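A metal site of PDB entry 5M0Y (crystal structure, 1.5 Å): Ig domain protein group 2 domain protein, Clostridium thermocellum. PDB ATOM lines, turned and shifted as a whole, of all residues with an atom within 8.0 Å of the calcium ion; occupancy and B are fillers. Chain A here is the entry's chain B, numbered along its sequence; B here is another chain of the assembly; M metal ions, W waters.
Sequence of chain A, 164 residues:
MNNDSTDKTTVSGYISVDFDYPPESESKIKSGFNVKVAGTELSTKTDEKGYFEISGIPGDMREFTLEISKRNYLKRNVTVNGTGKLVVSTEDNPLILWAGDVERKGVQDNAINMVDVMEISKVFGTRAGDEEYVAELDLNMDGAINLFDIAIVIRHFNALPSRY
N of Val 102 lies close to OD1 of Asp 116, at 2.8 Å. The side-chain carboxylate of Asp 101 lies within hydrogen-bond range of the backbone NH of Asn 110 (3.0 Å). O of Asp 101 lies within hydrogen-bond range of NE2 of Gln 108 (3.0 Å). The backbone NH (N) of Asp 101 sits at hydrogen-bond distance from the backbone carbonyl oxygen (O) of Asn 72 (3.2 Å). The side-chain carboxylate (OD2) of Asp 116 lies close to the backbone NH (N) of Asn 113 (2.8 Å).
Within 4 Å of the calcium ion: Asp 101, Asp 109, Ala 111 and Asp 116.
The calcium ion is bound by water W1 (2.3 Å), the side-chain carboxylate (OD1) of Asp 101 (2.3 Å), the backbone carbonyl oxygen (O) of Ala 111 (2.3 Å), the side-chain carboxylate (OD1) of Asp 109 (2.4 Å), the side-chain carboxylate (OD1) of Asp 116 (2.5 Å), water W2 (2.5 Å) and the side-chain carboxylate (OD2) of Asp 116 (2.6 Å).
Water W2 bridges O of Val 102 and N of Asp 109. Water W1 bridges OD2 of Asp 109 (2.7 Å) and OD1 of Asn 113 (2.7 Å).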
ATOM      1  N   ASN A  72     -18.008  10.634   5.451  1.00  0.00           N
ATOM      2  CA  ASN A  72     -18.955  11.692   5.824  1.00  0.00           C
ATOM      3  C   ASN A  72     -18.930  12.138   7.299  1.00  0.00           C
ATOM      4  O   ASN A  72     -19.814  12.866   7.739  1.00  0.00           O
ATOM      5  CB  ASN A  72     -20.385  11.386   5.337  1.00  0.00           C
ATOM      6  CG  ASN A  72     -20.464  11.240   3.820  1.00  0.00           C
ATOM      7  OD1 ASN A  72     -19.573  11.694   3.099  1.00  0.00           O
ATOM      8  ND2 ASN A  72     -21.519  10.599   3.337  1.00  0.00           N
ATOM      9  N   TYR A  73     -17.885  11.739   8.037  1.00  0.00           N
ATOM     10  CA  TYR A  73     -17.652  12.224   9.391  1.00  0.00           C
ATOM     11  C   TYR A  73     -16.427  13.120   9.446  1.00  0.00           C
ATOM     12  O   TYR A  73     -15.480  12.951   8.669  1.00  0.00           O
ATOM     13  CB  TYR A  73     -17.459  11.042  10.371  1.00  0.00           C
ATOM     14  CG  TYR A  73     -18.768  10.388  10.747  1.00  0.00           C
ATOM     15  CD1 TYR A  73     -19.485   9.622   9.834  1.00  0.00           C
ATOM     16  CD2 TYR A  73     -19.323  10.555  12.019  1.00  0.00           C
ATOM     17  CE1 TYR A  73     -20.698   9.045  10.153  1.00  0.00           C
ATOM     18  CE2 TYR A  73     -20.533   9.984  12.360  1.00  0.00           C
ATOM     19  CZ  TYR A  73     -21.227   9.230  11.425  1.00  0.00           C
ATOM     20  OH  TYR A  73     -22.432   8.663  11.749  1.00  0.00           O
ATOM     21  N   LEU A  74     -16.454  14.060  10.396  1.00  0.00           N
ATOM     22  CA  LEU A  74     -15.309  14.926  10.637  1.00  0.00           C
ATOM     23  C   LEU A  74     -14.242  14.096  11.342  1.00  0.00           C
ATOM     24  O   LEU A  74     -14.478  13.562  12.448  1.00  0.00           O
ATOM     25  CB  LEU A  74     -15.710  16.139  11.493  1.00  0.00           C
ATOM     26  CG  LEU A  74     -14.628  17.190  11.721  1.00  0.00           C
ATOM     27  CD1 LEU A  74     -14.245  17.880  10.421  1.00  0.00           C
ATOM     28  CD2 LEU A  74     -15.092  18.204  12.760  1.00  0.00           C
ATOM     29  N   GLY A 100     -21.199  14.755   9.316  1.00  0.00           N
ATOM     30  CA  GLY A 100     -21.483  15.938   8.496  1.00  0.00           C
ATOM     31  C   GLY A 100     -20.304  16.622   7.828  1.00  0.00           C
ATOM     32  O   GLY A 100     -20.487  17.723   7.315  1.00  0.00           O
ATOM     33  N   ASP A 101     -19.113  16.015   7.815  1.00  0.00           N
ATOM     34  CA  ASP A 101     -18.076  16.459   6.880  1.00  0.00           C
ATOM     35  C   ASP A 101     -18.216  15.546   5.663  1.00  0.00           C
ATOM     36  O   ASP A 101     -17.600  14.488   5.590  1.00  0.00           O
ATOM     37  CB  ASP A 101     -16.659  16.423   7.465  1.00  0.00           C
ATOM     38  CG  ASP A 101     -15.619  16.936   6.487  1.00  0.00           C
ATOM     39  OD1 ASP A 101     -15.968  17.704   5.549  1.00  0.00           O
ATOM     40  OD2 ASP A 101     -14.427  16.584   6.629  1.00  0.00           O
ATOM     41  N   VAL A 102     -19.036  15.989   4.711  1.00  0.00           N
ATOM     42  CA  VAL A 102     -19.556  15.128   3.669  1.00  0.00           C
ATOM     43  C   VAL A 102     -18.599  15.102   2.480  1.00  0.00           C
ATOM     44  O   VAL A 102     -18.068  16.136   2.061  1.00  0.00           O
ATOM     45  CB  VAL A 102     -20.967  15.582   3.234  1.00  0.00           C
ATOM     46  CG1 VAL A 102     -21.551  14.648   2.210  1.00  0.00           C
ATOM     47  CG2 VAL A 102     -21.896  15.657   4.439  1.00  0.00           C
ATOM     48  N   GLU A 103     -18.374  13.904   1.936  1.00  0.00           N
ATOM     49  CA  GLU A 103     -17.565  13.720   0.735  1.00  0.00           C
ATOM     50  C   GLU A 103     -18.239  14.352  -0.478  1.00  0.00           C
ATOM     51  O   GLU A 103     -19.464  14.292  -0.621  1.00  0.00           O
ATOM     52  CB  GLU A 103     -17.312  12.242   0.448  1.00  0.00           C
ATOM     53  CG  GLU A 103     -16.415  11.572   1.475  1.00  0.00           C
ATOM     54  CD  GLU A 103     -15.833  10.241   1.027  1.00  0.00           C
ATOM     55  OE1 GLU A 103     -16.257   9.703  -0.013  1.00  0.00           O
ATOM     56  OE2 GLU A 103     -14.929   9.736   1.738  1.00  0.00           O
ATOM     57  N   ARG A 104     -17.418  14.958  -1.329  1.00  0.00           N
ATOM     58  CA  ARG A 104     -17.818  15.373  -2.667  1.00  0.00           C
ATOM     59  C   ARG A 104     -16.742  14.881  -3.610  1.00  0.00           C
ATOM     60  O   ARG A 104     -15.573  15.231  -3.449  1.00  0.00           O
ATOM     61  CB  ARG A 104     -17.936  16.897  -2.744  1.00  0.00           C
ATOM     62  CG  ARG A 104     -19.211  17.439  -2.103  1.00  0.00           C
ATOM     63  CD  ARG A 104     -19.117  18.943  -1.942  1.00  0.00           C
ATOM     64  NE  ARG A 104     -20.363  19.572  -1.498  1.00  0.00           N
ATOM     65  CZ  ARG A 104     -21.293  20.139  -2.288  1.00  0.00           C
ATOM     66  NH1 ARG A 104     -21.185  20.155  -3.613  1.00  0.00           N
ATOM     67  NH2 ARG A 104     -22.352  20.702  -1.726  1.00  0.00           N
ATOM     68  N   VAL A 107     -13.838  13.402  -1.724  1.00  0.00           N
ATOM     69  CA  VAL A 107     -12.944  14.312  -0.993  1.00  0.00           C
ATOM     70  C   VAL A 107     -13.710  15.068   0.093  1.00  0.00           C
ATOM     71  O   VAL A 107     -14.770  15.647  -0.186  1.00  0.00           O
ATOM     72  CB  VAL A 107     -12.288  15.335  -1.937  1.00  0.00           C
ATOM     73  CG1 VAL A 107     -11.328  16.249  -1.167  1.00  0.00           C
ATOM     74  CG2 VAL A 107     -11.558  14.626  -3.077  1.00  0.00           C
ATOM     75  N   GLN A 108     -13.175  15.063   1.313  1.00  0.00           N
ATOM     76  CA  GLN A 108     -13.681  15.864   2.433  1.00  0.00           C
ATOM     77  C   GLN A 108     -12.720  17.019   2.671  1.00  0.00           C
ATOM     78  O   GLN A 108     -11.526  16.920   2.346  1.00  0.00           O
ATOM     79  CB  GLN A 108     -13.830  15.010   3.703  1.00  0.00           C
ATOM     80  CG  GLN A 108     -14.773  13.834   3.496  1.00  0.00           C
ATOM     81  CD  GLN A 108     -15.072  12.952   4.714  1.00  0.00           C
ATOM     82  OE1 GLN A 108     -15.590  11.846   4.558  1.00  0.00           O
ATOM     83  NE2 GLN A 108     -14.794  13.432   5.906  1.00  0.00           N
ATOM     84  N   ASP A 109     -13.219  18.128   3.228  1.00  0.00           N
ATOM     85  CA  ASP A 109     -12.376  19.310   3.487  1.00  0.00           C
ATOM     86  C   ASP A 109     -12.087  19.575   4.974  1.00  0.00           C
ATOM     87  O   ASP A 109     -11.559  20.626   5.317  1.00  0.00           O
ATOM     88  CB  ASP A 109     -12.944  20.541   2.776  1.00  0.00           C
ATOM     89  CG  ASP A 109     -14.307  20.966   3.286  1.00  0.00           C
ATOM     90  OD1 ASP A 109     -14.842  20.379   4.258  1.00  0.00           O
ATOM     91  OD2 ASP A 109     -14.892  21.910   2.705  1.00  0.00           O
ATOM     92  N   ASN A 110     -12.435  18.624   5.842  1.00  0.00           N
ATOM     93  CA  ASN A 110     -12.107  18.707   7.260  1.00  0.00           C
ATOM     94  C   ASN A 110     -12.732  19.914   7.961  1.00  0.00           C
ATOM     95  O   ASN A 110     -12.141  20.517   8.857  1.00  0.00           O
ATOM     96  CB  ASN A 110     -10.579  18.656   7.464  1.00  0.00           C
ATOM     97  CG  ASN A 110      -9.955  17.422   6.837  1.00  0.00           C
ATOM     98  OD1 ASN A 110     -10.447  16.294   7.012  1.00  0.00           O
ATOM     99  ND2 ASN A 110      -8.867  17.609   6.116  1.00  0.00           N
ATOM    100  N   ALA A 111     -13.949  20.261   7.525  1.00  0.00           N
ATOM    101  CA  ALA A 111     -14.756  21.299   8.158  1.00  0.00           C
ATOM    102  C   ALA A 111     -16.209  20.914   7.978  1.00  0.00           C
ATOM    103  O   ALA A 111     -16.560  20.326   6.959  1.00  0.00           O
ATOM    104  CB  ALA A 111     -14.499  22.656   7.519  1.00  0.00           C
ATOM    105  N   ILE A 112     -17.048  21.210   8.970  1.00  0.00           N
ATOM    106  CA  ILE A 112     -18.499  21.021   8.825  1.00  0.00           C
ATOM    107  C   ILE A 112     -19.094  22.405   8.569  1.00  0.00           C
ATOM    108  O   ILE A 112     -18.966  23.277   9.404  1.00  0.00           O
ATOM    109  CB  ILE A 112     -19.122  20.411  10.081  1.00  0.00           C
ATOM    110  CG1 ILE A 112     -18.513  19.005  10.317  1.00  0.00           C
ATOM    111  CG2 ILE A 112     -20.638  20.349   9.944  1.00  0.00           C
ATOM    112  CD1 ILE A 112     -19.070  18.260  11.520  1.00  0.00           C
ATOM    113  N   ASN A 113     -19.721  22.609   7.411  1.00  0.00           N
ATOM    114  CA  ASN A 113     -20.288  23.926   7.108  1.00  0.00           C
ATOM    115  C   ASN A 113     -21.373  23.813   6.035  1.00  0.00           C
ATOM    116  O   ASN A 113     -21.856  22.708   5.766  1.00  0.00           O
ATOM    117  CB  ASN A 113     -19.146  24.894   6.710  1.00  0.00           C
ATOM    118  CG  ASN A 113     -18.368  24.438   5.496  1.00  0.00           C
ATOM    119  OD1 ASN A 113     -18.902  23.753   4.634  1.00  0.00           O
ATOM    120  ND2 ASN A 113     -17.095  24.834   5.420  1.00  0.00           N
ATOM    121  N   MET A 114     -21.731  24.931   5.406  1.00  0.00           N
ATOM    122  CA  MET A 114     -22.866  24.923   4.476  1.00  0.00           C
ATOM    123  C   MET A 114     -22.628  24.063   3.243  1.00  0.00           C
ATOM    124  O   MET A 114     -23.583  23.550   2.674  1.00  0.00           O
ATOM    125  CB  MET A 114     -23.238  26.341   4.066  1.00  0.00           C
ATOM    126  CG  MET A 114     -24.654  26.487   3.572  1.00  0.00           C
ATOM    127  SD  MET A 114     -25.837  26.040   4.861  1.00  0.00           S
ATOM    128  CE  MET A 114     -27.361  26.619   4.109  1.00  0.00           C
ATOM    129  N   VAL A 115     -21.378  23.884   2.833  1.00  0.00           N
ATOM    130  CA  VAL A 115     -21.065  23.000   1.703  1.00  0.00           C
ATOM    131  C   VAL A 115     -21.618  21.599   1.993  1.00  0.00           C
ATOM    132  O   VAL A 115     -22.208  20.955   1.119  1.00  0.00           O
ATOM    133  CB  VAL A 115     -19.544  22.950   1.414  1.00  0.00           C
ATOM    134  CG1 VAL A 115     -19.239  21.961   0.291  1.00  0.00           C
ATOM    135  CG2 VAL A 115     -19.002  24.339   1.068  1.00  0.00           C
ATOM    136  N   ASP A 116     -21.484  21.162   3.241  1.00  0.00           N
ATOM    137  CA  ASP A 116     -21.990  19.832   3.644  1.00  0.00           C
ATOM    138  C   ASP A 116     -23.496  19.750   3.666  1.00  0.00           C
ATOM    139  O   ASP A 116     -24.064  18.780   3.190  1.00  0.00           O
ATOM    140  CB  ASP A 116     -21.410  19.480   4.997  1.00  0.00           C
ATOM    141  CG  ASP A 116     -19.890  19.535   4.984  1.00  0.00           C
ATOM    142  OD1 ASP A 116     -19.280  18.743   4.240  1.00  0.00           O
ATOM    143  OD2 ASP A 116     -19.309  20.387   5.675  1.00  0.00           O
ATOM    144  N   VAL A 117     -24.147  20.791   4.179  1.00  0.00           N
ATOM    145  CA  VAL A 117     -25.608  20.893   4.170  1.00  0.00           C
ATOM    146  C   VAL A 117     -26.130  20.781   2.736  1.00  0.00           C
ATOM    147  O   VAL A 117     -27.094  20.058   2.481  1.00  0.00           O
ATOM    148  CB  VAL A 117     -26.084  22.225   4.793  1.00  0.00           C
ATOM    149  CG1 VAL A 117     -27.566  22.460   4.558  1.00  0.00           C
ATOM    150  CG2 VAL A 117     -25.739  22.266   6.286  1.00  0.00           C
ATOM    151  N   VAL A 153     -25.974  17.884  10.875  1.00  0.00           N
ATOM    152  CA  VAL A 153     -24.855  18.668  10.353  1.00  0.00           C
ATOM    153  C   VAL A 153     -24.788  20.017  11.079  1.00  0.00           C
ATOM    154  O   VAL A 153     -23.717  20.436  11.552  1.00  0.00           O
ATOM    155  CB  VAL A 153     -24.960  18.876   8.817  1.00  0.00           C
ATOM    156  CG1 VAL A 153     -23.812  19.732   8.303  1.00  0.00           C
ATOM    157  CG2 VAL A 153     -24.969  17.533   8.103  1.00  0.00           C
ATOM    158  N   ALA A 159     -17.536  23.410  12.685  1.00  0.00           N
ATOM    159  CA  ALA A 159     -16.565  22.596  13.435  1.00  0.00           C
ATOM    160  C   ALA A 159     -15.359  22.233  12.590  1.00  0.00           C
ATOM    161  O   ALA A 159     -15.474  21.971  11.398  1.00  0.00           O
ATOM    162  CB  ALA A 159     -17.222  21.333  13.967  1.00  0.00           C
ATOM    163  N   SER B 141     -13.054  27.920   9.335  1.00  0.00           N
ATOM    164  CA  SER B 141     -14.226  27.052   9.235  1.00  0.00           C
ATOM    165  C   SER B 141     -14.814  26.973   7.822  1.00  0.00           C
ATOM    166  O   SER B 141     -15.688  26.153   7.574  1.00  0.00           O
ATOM    167  CB  SER B 141     -15.308  27.448  10.244  1.00  0.00           C
ATOM    168  OG  SER B 141     -15.985  28.613   9.837  1.00  0.00           O
ATOM    169  N   PRO B 143     -12.925  26.489   4.537  1.00  0.00           N
ATOM    170  CA  PRO B 143     -11.824  26.299   3.595  1.00  0.00           C
ATOM    171  C   PRO B 143     -12.314  26.356   2.141  1.00  0.00           C
ATOM    172  O   PRO B 143     -13.376  25.841   1.826  1.00  0.00           O
ATOM    173  CB  PRO B 143     -11.285  24.895   3.941  1.00  0.00           C
ATOM    174  CG  PRO B 143     -12.424  24.220   4.605  1.00  0.00           C
ATOM    175  CD  PRO B 143     -13.151  25.286   5.362  1.00  0.00           C
HETATM  176 CA    CA M   1     -17.038  19.626   4.779  1.00  0.00          CA
HETATM  177  O   HOH W   1     -17.397  21.662   3.710  1.00  0.00           O
HETATM  178  O   HOH W   2     -16.587  18.398   2.660  1.00  0.00           O
